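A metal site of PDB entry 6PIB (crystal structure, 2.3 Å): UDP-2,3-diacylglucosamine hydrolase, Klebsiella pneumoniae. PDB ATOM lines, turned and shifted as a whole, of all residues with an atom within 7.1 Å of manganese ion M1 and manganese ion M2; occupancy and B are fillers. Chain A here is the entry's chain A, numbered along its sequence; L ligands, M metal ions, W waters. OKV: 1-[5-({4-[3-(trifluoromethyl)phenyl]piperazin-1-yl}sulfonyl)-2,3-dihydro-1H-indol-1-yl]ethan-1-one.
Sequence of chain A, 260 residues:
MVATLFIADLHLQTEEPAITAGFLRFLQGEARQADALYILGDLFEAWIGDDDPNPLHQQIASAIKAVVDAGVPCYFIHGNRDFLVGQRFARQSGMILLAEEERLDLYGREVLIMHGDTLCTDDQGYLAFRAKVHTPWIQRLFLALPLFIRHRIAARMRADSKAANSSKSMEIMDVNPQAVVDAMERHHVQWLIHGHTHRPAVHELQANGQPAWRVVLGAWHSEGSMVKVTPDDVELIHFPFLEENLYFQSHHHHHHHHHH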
ATOM      1  N   ALA A   8     -22.440  15.885  28.002  1.00  0.00           N
ATOM      2  CA  ALA A   8     -22.230  17.320  28.109  1.00  0.00           C
ATOM      3  C   ALA A   8     -22.936  17.817  29.367  1.00  0.00           C
ATOM      4  O   ALA A   8     -23.763  17.120  29.958  1.00  0.00           O
ATOM      5  CB  ALA A   8     -22.744  18.075  26.880  1.00  0.00           C
ATOM      6  N   ASP A   9     -22.576  19.042  29.777  1.00  0.00           N
ATOM      7  CA  ASP A   9     -23.254  19.760  30.854  1.00  0.00           C
ATOM      8  C   ASP A   9     -23.221  18.976  32.162  1.00  0.00           C
ATOM      9  O   ASP A   9     -24.239  18.794  32.835  1.00  0.00           O
ATOM     10  CB  ASP A   9     -24.685  20.111  30.455  1.00  0.00           C
ATOM     11  CG  ASP A   9     -24.739  21.025  29.245  1.00  0.00           C
ATOM     12  OD1 ASP A   9     -24.223  22.160  29.334  1.00  0.00           O
ATOM     13  OD2 ASP A   9     -25.299  20.610  28.206  1.00  0.00           O
ATOM     14  N   LEU A  10     -22.027  18.508  32.523  1.00  0.00           N
ATOM     15  CA  LEU A  10     -21.864  17.865  33.819  1.00  0.00           C
ATOM     16  C   LEU A  10     -21.703  18.893  34.942  1.00  0.00           C
ATOM     17  O   LEU A  10     -22.123  18.624  36.078  1.00  0.00           O
ATOM     18  CB  LEU A  10     -20.662  16.922  33.797  1.00  0.00           C
ATOM     19  CG  LEU A  10     -20.894  15.560  33.144  1.00  0.00           C
ATOM     20  CD1 LEU A  10     -20.772  15.647  31.629  1.00  0.00           C
ATOM     21  CD2 LEU A  10     -19.919  14.545  33.708  1.00  0.00           C
ATOM     22  N   HIS A  11     -21.111  20.046  34.635  1.00  0.00           N
ATOM     23  CA  HIS A  11     -20.925  21.122  35.602  1.00  0.00           C
ATOM     24  C   HIS A  11     -20.235  20.623  36.863  1.00  0.00           C
ATOM     25  O   HIS A  11     -20.654  20.897  37.992  1.00  0.00           O
ATOM     26  CB  HIS A  11     -22.268  21.787  35.933  1.00  0.00           C
ATOM     27  CG  HIS A  11     -22.872  22.533  34.786  1.00  0.00           C
ATOM     28  ND1 HIS A  11     -22.572  23.854  34.517  1.00  0.00           N
ATOM     29  CD2 HIS A  11     -23.751  22.142  33.829  1.00  0.00           C
ATOM     30  CE1 HIS A  11     -23.246  24.251  33.449  1.00  0.00           C
ATOM     31  NE2 HIS A  11     -23.960  23.224  33.013  1.00  0.00           N
ATOM     32  N   LEU A  40     -19.347  17.425  25.042  1.00  0.00           N
ATOM     33  CA  LEU A  40     -19.770  18.602  24.292  1.00  0.00           C
ATOM     34  C   LEU A  40     -19.956  19.833  25.183  1.00  0.00           C
ATOM     35  O   LEU A  40     -21.004  20.482  25.158  1.00  0.00           O
ATOM     36  CB  LEU A  40     -21.048  18.298  23.519  1.00  0.00           C
ATOM     37  CG  LEU A  40     -21.030  17.046  22.642  1.00  0.00           C
ATOM     38  CD1 LEU A  40     -22.323  16.924  21.849  1.00  0.00           C
ATOM     39  CD2 LEU A  40     -19.829  17.056  21.707  1.00  0.00           C
ATOM     40  N   GLY A  41     -18.942  20.161  25.972  1.00  0.00           N
ATOM     41  CA  GLY A  41     -18.938  21.407  26.702  1.00  0.00           C
ATOM     42  C   GLY A  41     -19.522  21.285  28.103  1.00  0.00           C
ATOM     43  O   GLY A  41     -20.271  20.371  28.421  1.00  0.00           O
ATOM     44  N   ASP A  42     -19.156  22.266  28.936  1.00  0.00           N
ATOM     45  CA  ASP A  42     -19.626  22.365  30.313  1.00  0.00           C
ATOM     46  C   ASP A  42     -19.304  21.099  31.111  1.00  0.00           C
ATOM     47  O   ASP A  42     -20.108  20.636  31.921  1.00  0.00           O
ATOM     48  CB  ASP A  42     -21.129  22.670  30.362  1.00  0.00           C
ATOM     49  CG  ASP A  42     -21.436  24.109  29.997  1.00  0.00           C
ATOM     50  OD1 ASP A  42     -20.480  24.848  29.659  1.00  0.00           O
ATOM     51  OD2 ASP A  42     -22.623  24.498  30.031  1.00  0.00           O
ATOM     52  N   GLU A  45     -18.016  23.364  35.973  1.00  0.00           N
ATOM     53  CA  GLU A  45     -18.845  24.532  36.248  1.00  0.00           C
ATOM     54  C   GLU A  45     -18.086  25.829  35.987  1.00  0.00           C
ATOM     55  O   GLU A  45     -18.688  26.840  35.623  1.00  0.00           O
ATOM     56  CB  GLU A  45     -19.361  24.480  37.681  1.00  0.00           C
ATOM     57  CG  GLU A  45     -20.056  25.738  38.177  1.00  0.00           C
ATOM     58  CD  GLU A  45     -21.355  26.032  37.444  1.00  0.00           C
ATOM     59  OE1 GLU A  45     -21.916  25.100  36.829  1.00  0.00           O
ATOM     60  OE2 GLU A  45     -21.814  27.192  37.484  1.00  0.00           O
ATOM     61  N   GLY A  79     -17.501  24.534  26.270  1.00  0.00           N
ATOM     62  CA  GLY A  79     -18.801  25.069  26.612  1.00  0.00           C
ATOM     63  C   GLY A  79     -18.719  26.531  27.004  1.00  0.00           C
ATOM     64  O   GLY A  79     -17.675  27.169  26.923  1.00  0.00           O
ATOM     65  N   ASN A  80     -19.864  27.054  27.441  1.00  0.00           N
ATOM     66  CA  ASN A  80     -19.902  28.443  27.898  1.00  0.00           C
ATOM     67  C   ASN A  80     -19.282  28.623  29.275  1.00  0.00           C
ATOM     68  O   ASN A  80     -18.899  29.737  29.625  1.00  0.00           O
ATOM     69  CB  ASN A  80     -21.346  28.957  27.909  1.00  0.00           C
ATOM     70  CG  ASN A  80     -22.267  28.116  28.760  1.00  0.00           C
ATOM     71  OD1 ASN A  80     -22.704  27.042  28.341  1.00  0.00           O
ATOM     72  ND2 ASN A  80     -22.572  28.591  29.960  1.00  0.00           N
ATOM     73  N   ARG A  81     -19.156  27.549  30.046  1.00  0.00           N
ATOM     74  CA  ARG A  81     -18.564  27.624  31.387  1.00  0.00           C
ATOM     75  C   ARG A  81     -17.064  27.380  31.373  1.00  0.00           C
ATOM     76  O   ARG A  81     -16.325  28.039  32.101  1.00  0.00           O
ATOM     77  CB  ARG A  81     -19.245  26.624  32.324  1.00  0.00           C
ATOM     78  CG  ARG A  81     -20.764  26.729  32.365  1.00  0.00           C
ATOM     79  CD  ARG A  81     -21.217  28.045  32.964  1.00  0.00           C
ATOM     80  NE  ARG A  81     -20.589  28.296  34.261  1.00  0.00           N
ATOM     81  CZ  ARG A  81     -20.952  29.275  35.086  1.00  0.00           C
ATOM     82  NH1 ARG A  81     -21.936  30.097  34.750  1.00  0.00           N
ATOM     83  NH2 ARG A  81     -20.331  29.432  36.247  1.00  0.00           N
ATOM     84  N   HIS A 115     -21.640  22.661  21.267  1.00  0.00           N
ATOM     85  CA  HIS A 115     -22.140  22.814  22.621  1.00  0.00           C
ATOM     86  C   HIS A 115     -23.606  23.244  22.625  1.00  0.00           C
ATOM     87  O   HIS A 115     -24.393  22.753  23.446  1.00  0.00           O
ATOM     88  CB  HIS A 115     -21.301  23.810  23.412  1.00  0.00           C
ATOM     89  CG  HIS A 115     -21.776  23.999  24.819  1.00  0.00           C
ATOM     90  ND1 HIS A 115     -21.829  22.973  25.737  1.00  0.00           N
ATOM     91  CD2 HIS A 115     -22.243  25.101  25.463  1.00  0.00           C
ATOM     92  CE1 HIS A 115     -22.297  23.431  26.887  1.00  0.00           C
ATOM     93  NE2 HIS A 115     -22.553  24.722  26.743  1.00  0.00           N
ATOM     94  N   GLY A 116     -23.986  24.143  21.719  1.00  0.00           N
ATOM     95  CA  GLY A 116     -25.355  24.585  21.578  1.00  0.00           C
ATOM     96  C   GLY A 116     -25.600  26.009  22.011  1.00  0.00           C
ATOM     97  O   GLY A 116     -26.660  26.570  21.684  1.00  0.00           O
ATOM     98  N   ASP A 117     -24.667  26.625  22.744  1.00  0.00           N
ATOM     99  CA  ASP A 117     -24.881  27.984  23.220  1.00  0.00           C
ATOM    100  C   ASP A 117     -24.923  28.988  22.069  1.00  0.00           C
ATOM    101  O   ASP A 117     -25.630  29.996  22.158  1.00  0.00           O
ATOM    102  CB  ASP A 117     -23.797  28.366  24.228  1.00  0.00           C
ATOM    103  CG  ASP A 117     -22.409  28.379  23.606  1.00  0.00           C
ATOM    104  OD1 ASP A 117     -22.008  27.348  23.028  1.00  0.00           O
ATOM    105  OD2 ASP A 117     -21.718  29.414  23.712  1.00  0.00           O
ATOM    106  N   TYR A 126     -26.365  37.342  26.625  1.00  0.00           N
ATOM    107  CA  TYR A 126     -25.326  36.320  26.628  1.00  0.00           C
ATOM    108  C   TYR A 126     -24.410  36.451  25.424  1.00  0.00           C
ATOM    109  O   TYR A 126     -23.197  36.233  25.529  1.00  0.00           O
ATOM    110  CB  TYR A 126     -25.929  34.919  26.675  1.00  0.00           C
ATOM    111  CG  TYR A 126     -24.929  33.834  26.358  1.00  0.00           C
ATOM    112  CD1 TYR A 126     -23.949  33.478  27.276  1.00  0.00           C
ATOM    113  CD2 TYR A 126     -24.935  33.179  25.130  1.00  0.00           C
ATOM    114  CE1 TYR A 126     -23.012  32.491  26.988  1.00  0.00           C
ATOM    115  CE2 TYR A 126     -24.019  32.196  24.835  1.00  0.00           C
ATOM    116  CZ  TYR A 126     -23.057  31.855  25.771  1.00  0.00           C
ATOM    117  OH  TYR A 126     -22.140  30.872  25.476  1.00  0.00           O
ATOM    118  N   GLY A 195     -25.801  20.300  23.590  1.00  0.00           N
ATOM    119  CA  GLY A 195     -26.319  20.360  24.949  1.00  0.00           C
ATOM    120  C   GLY A 195     -26.718  21.766  25.348  1.00  0.00           C
ATOM    121  O   GLY A 195     -27.581  22.386  24.706  1.00  0.00           O
ATOM    122  N   HIS A 196     -26.114  22.274  26.427  1.00  0.00           N
ATOM    123  CA  HIS A 196     -26.283  23.645  26.903  1.00  0.00           C
ATOM    124  C   HIS A 196     -27.683  23.933  27.435  1.00  0.00           C
ATOM    125  O   HIS A 196     -27.821  24.467  28.541  1.00  0.00           O
ATOM    126  CB  HIS A 196     -25.942  24.653  25.792  1.00  0.00           C
ATOM    127  CG  HIS A 196     -26.065  26.085  26.212  1.00  0.00           C
ATOM    128  ND1 HIS A 196     -25.195  26.682  27.091  1.00  0.00           N
ATOM    129  CD2 HIS A 196     -26.968  27.037  25.874  1.00  0.00           C
ATOM    130  CE1 HIS A 196     -25.548  27.937  27.275  1.00  0.00           C
ATOM    131  NE2 HIS A 196     -26.621  28.181  26.548  1.00  0.00           N
ATOM    132  N   THR A 197     -28.721  23.582  26.674  1.00  0.00           N
ATOM    133  CA  THR A 197     -30.083  23.952  27.041  1.00  0.00           C
ATOM    134  C   THR A 197     -30.668  23.097  28.162  1.00  0.00           C
ATOM    135  O   THR A 197     -31.697  23.476  28.726  1.00  0.00           O
ATOM    136  CB  THR A 197     -30.996  23.873  25.819  1.00  0.00           C
ATOM    137  OG1 THR A 197     -30.999  22.532  25.311  1.00  0.00           O
ATOM    138  CG2 THR A 197     -30.519  24.816  24.728  1.00  0.00           C
ATOM    139  N   HIS A 198     -30.047  21.963  28.496  1.00  0.00           N
ATOM    140  CA  HIS A 198     -30.482  21.101  29.601  1.00  0.00           C
ATOM    141  C   HIS A 198     -31.891  20.548  29.381  1.00  0.00           C
ATOM    142  O   HIS A 198     -32.637  20.321  30.335  1.00  0.00           O
ATOM    143  CB  HIS A 198     -30.406  21.824  30.940  1.00  0.00           C
ATOM    144  CG  HIS A 198     -29.017  22.208  31.356  1.00  0.00           C
ATOM    145  ND1 HIS A 198     -28.716  22.642  32.624  1.00  0.00           N
ATOM    146  CD2 HIS A 198     -27.854  22.214  30.660  1.00  0.00           C
ATOM    147  CE1 HIS A 198     -27.424  22.908  32.695  1.00  0.00           C
ATOM    148  NE2 HIS A 198     -26.876  22.656  31.515  1.00  0.00           N
ATOM    149  N   ALA A 219     -28.469  17.683  31.215  1.00  0.00           N
ATOM    150  CA  ALA A 219     -27.478  18.006  32.226  1.00  0.00           C
ATOM    151  C   ALA A 219     -27.468  16.937  33.315  1.00  0.00           C
ATOM    152  O   ALA A 219     -28.468  16.264  33.573  1.00  0.00           O
ATOM    153  CB  ALA A 219     -27.776  19.371  32.846  1.00  0.00           C
HETATM  154  C13 OKV L   1     -17.961  31.093  33.011  1.00  0.00           C
HETATM  155  C15 OKV L   1     -20.028  32.320  32.835  1.00  0.00           C
HETATM  156  C17 OKV L   1     -18.574  32.688  34.727  1.00  0.00           C
HETATM  157  C21 OKV L   1     -22.026  32.356  31.118  1.00  0.00           C
HETATM  158  C24 OKV L   1     -13.090  36.514  32.219  1.00  0.00           C
HETATM  159  C26 OKV L   1     -11.787  36.987  30.269  1.00  0.00           C
HETATM  160  C28 OKV L   1     -12.433  38.901  31.778  1.00  0.00           C
HETATM  161  C01 OKV L   1     -12.447  34.733  30.751  1.00  0.00           C
HETATM  162  C02 OKV L   1     -13.093  35.165  31.886  1.00  0.00           C
HETATM  163  C04 OKV L   1     -14.164  34.679  34.075  1.00  0.00           C
HETATM  164  C05 OKV L   1     -15.258  33.770  34.626  1.00  0.00           C
HETATM  165  C07 OKV L   1     -14.484  31.947  33.214  1.00  0.00           C
HETATM  166  C08 OKV L   1     -13.371  32.824  32.652  1.00  0.00           C
HETATM  167  C12 OKV L   1     -17.670  31.752  34.216  1.00  0.00           C
HETATM  168  C14 OKV L   1     -19.128  31.376  32.320  1.00  0.00           C
HETATM  169  C16 OKV L   1     -19.762  32.974  34.028  1.00  0.00           C
HETATM  170  C18 OKV L   1     -20.890  33.939  34.362  1.00  0.00           C
HETATM  171  C19 OKV L   1     -21.851  33.839  33.216  1.00  0.00           C
HETATM  172  C23 OKV L   1     -23.370  32.985  30.764  1.00  0.00           C
HETATM  173  C25 OKV L   1     -12.437  37.417  31.414  1.00  0.00           C
HETATM  174  C27 OKV L   1     -11.794  35.646  29.926  1.00  0.00           C
HETATM  175  F29 OKV L   1     -13.616  39.438  31.471  1.00  0.00           F
HETATM  176  F30 OKV L   1     -11.470  39.531  31.107  1.00  0.00           F
HETATM  177  F31 OKV L   1     -12.216  39.039  33.087  1.00  0.00           F
HETATM  178  N03 OKV L   1     -13.757  34.255  32.718  1.00  0.00           N
HETATM  179  N06 OKV L   1     -14.876  32.368  34.554  1.00  0.00           N
HETATM  180  N20 OKV L   1     -21.342  32.809  32.318  1.00  0.00           N
HETATM  181  O10 OKV L   1     -15.784  29.983  34.857  1.00  0.00           O
HETATM  182  O11 OKV L   1     -16.346  31.587  36.541  1.00  0.00           O
HETATM  183  O22 OKV L   1     -21.550  31.517  30.438  1.00  0.00           O
HETATM  184  S09 OKV L   1     -16.143  31.375  35.103  1.00  0.00           S
HETATM  185 MN    MN M   1     -23.766  25.476  28.490  1.00  0.00          MN
HETATM  186 MN    MN M   2     -24.782  23.139  30.875  1.00  0.00          MN
HETATM  187  O   HOH W   1     -25.174  25.060  30.031  1.00  0.00           O
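ND2 of Asn 80 lies within hydrogen-bond range of O22 of the ligand.
The side-chain carboxylate (OD2) of Asp 9 lies within hydrogen-bond range of the backbone NH (N) of His 196 (2.6 Å).
N of Asp 9 sits at hydrogen-bond distance from O of Gly 41.
The backbone NH (N) of Arg 81 sits at hydrogen-bond distance from the side-chain carboxylate (OD1) of Asp 42 (3.0 Å).
The backbone carbonyl oxygen of Asp 42 sits at hydrogen-bond distance from the backbone NH of Leu 10, 2.9 Å away.
The backbone carbonyl oxygen of His 115 sits at hydrogen-bond distance from the backbone NH of Gly 195 (2.8 Å).
A ring nitrogen (ND1) of His 115 is in hydrogen-bond range of the backbone carbonyl oxygen (O) of Leu 40, 2.7 Å away.
OE1 of Glu 45 is in hydrogen-bond range of ND1 of His 11 (2.7 Å).
The nearest printed residue that does not touch manganese ion M1 is His 11 (5.1 Å).
Of the 20 residues printed, 4 come within 4 Å of manganese ion M2.
Manganese ion M1 is bound by the side-chain amide oxygen (OD1) of Asn 80 (1.9 Å), water W1 (2.1 Å), the side-chain carboxylate (OD2) of Asp 42 (2.2 Å), a ring nitrogen (NE2) of His 115 (2.3 Å) and a ring nitrogen (ND1) of His 196 (2.3 Å).
Manganese ion M2 is bound by OD1 of Asp 9 (1.9 Å), water W1 (2.1 Å), NE2 of His 198 (2.2 Å), NE2 of His 11 (2.3 Å) and OD2 of Asp 42 (2.7 Å).
Manganese ion M2 has five donor atoms within binding distance.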
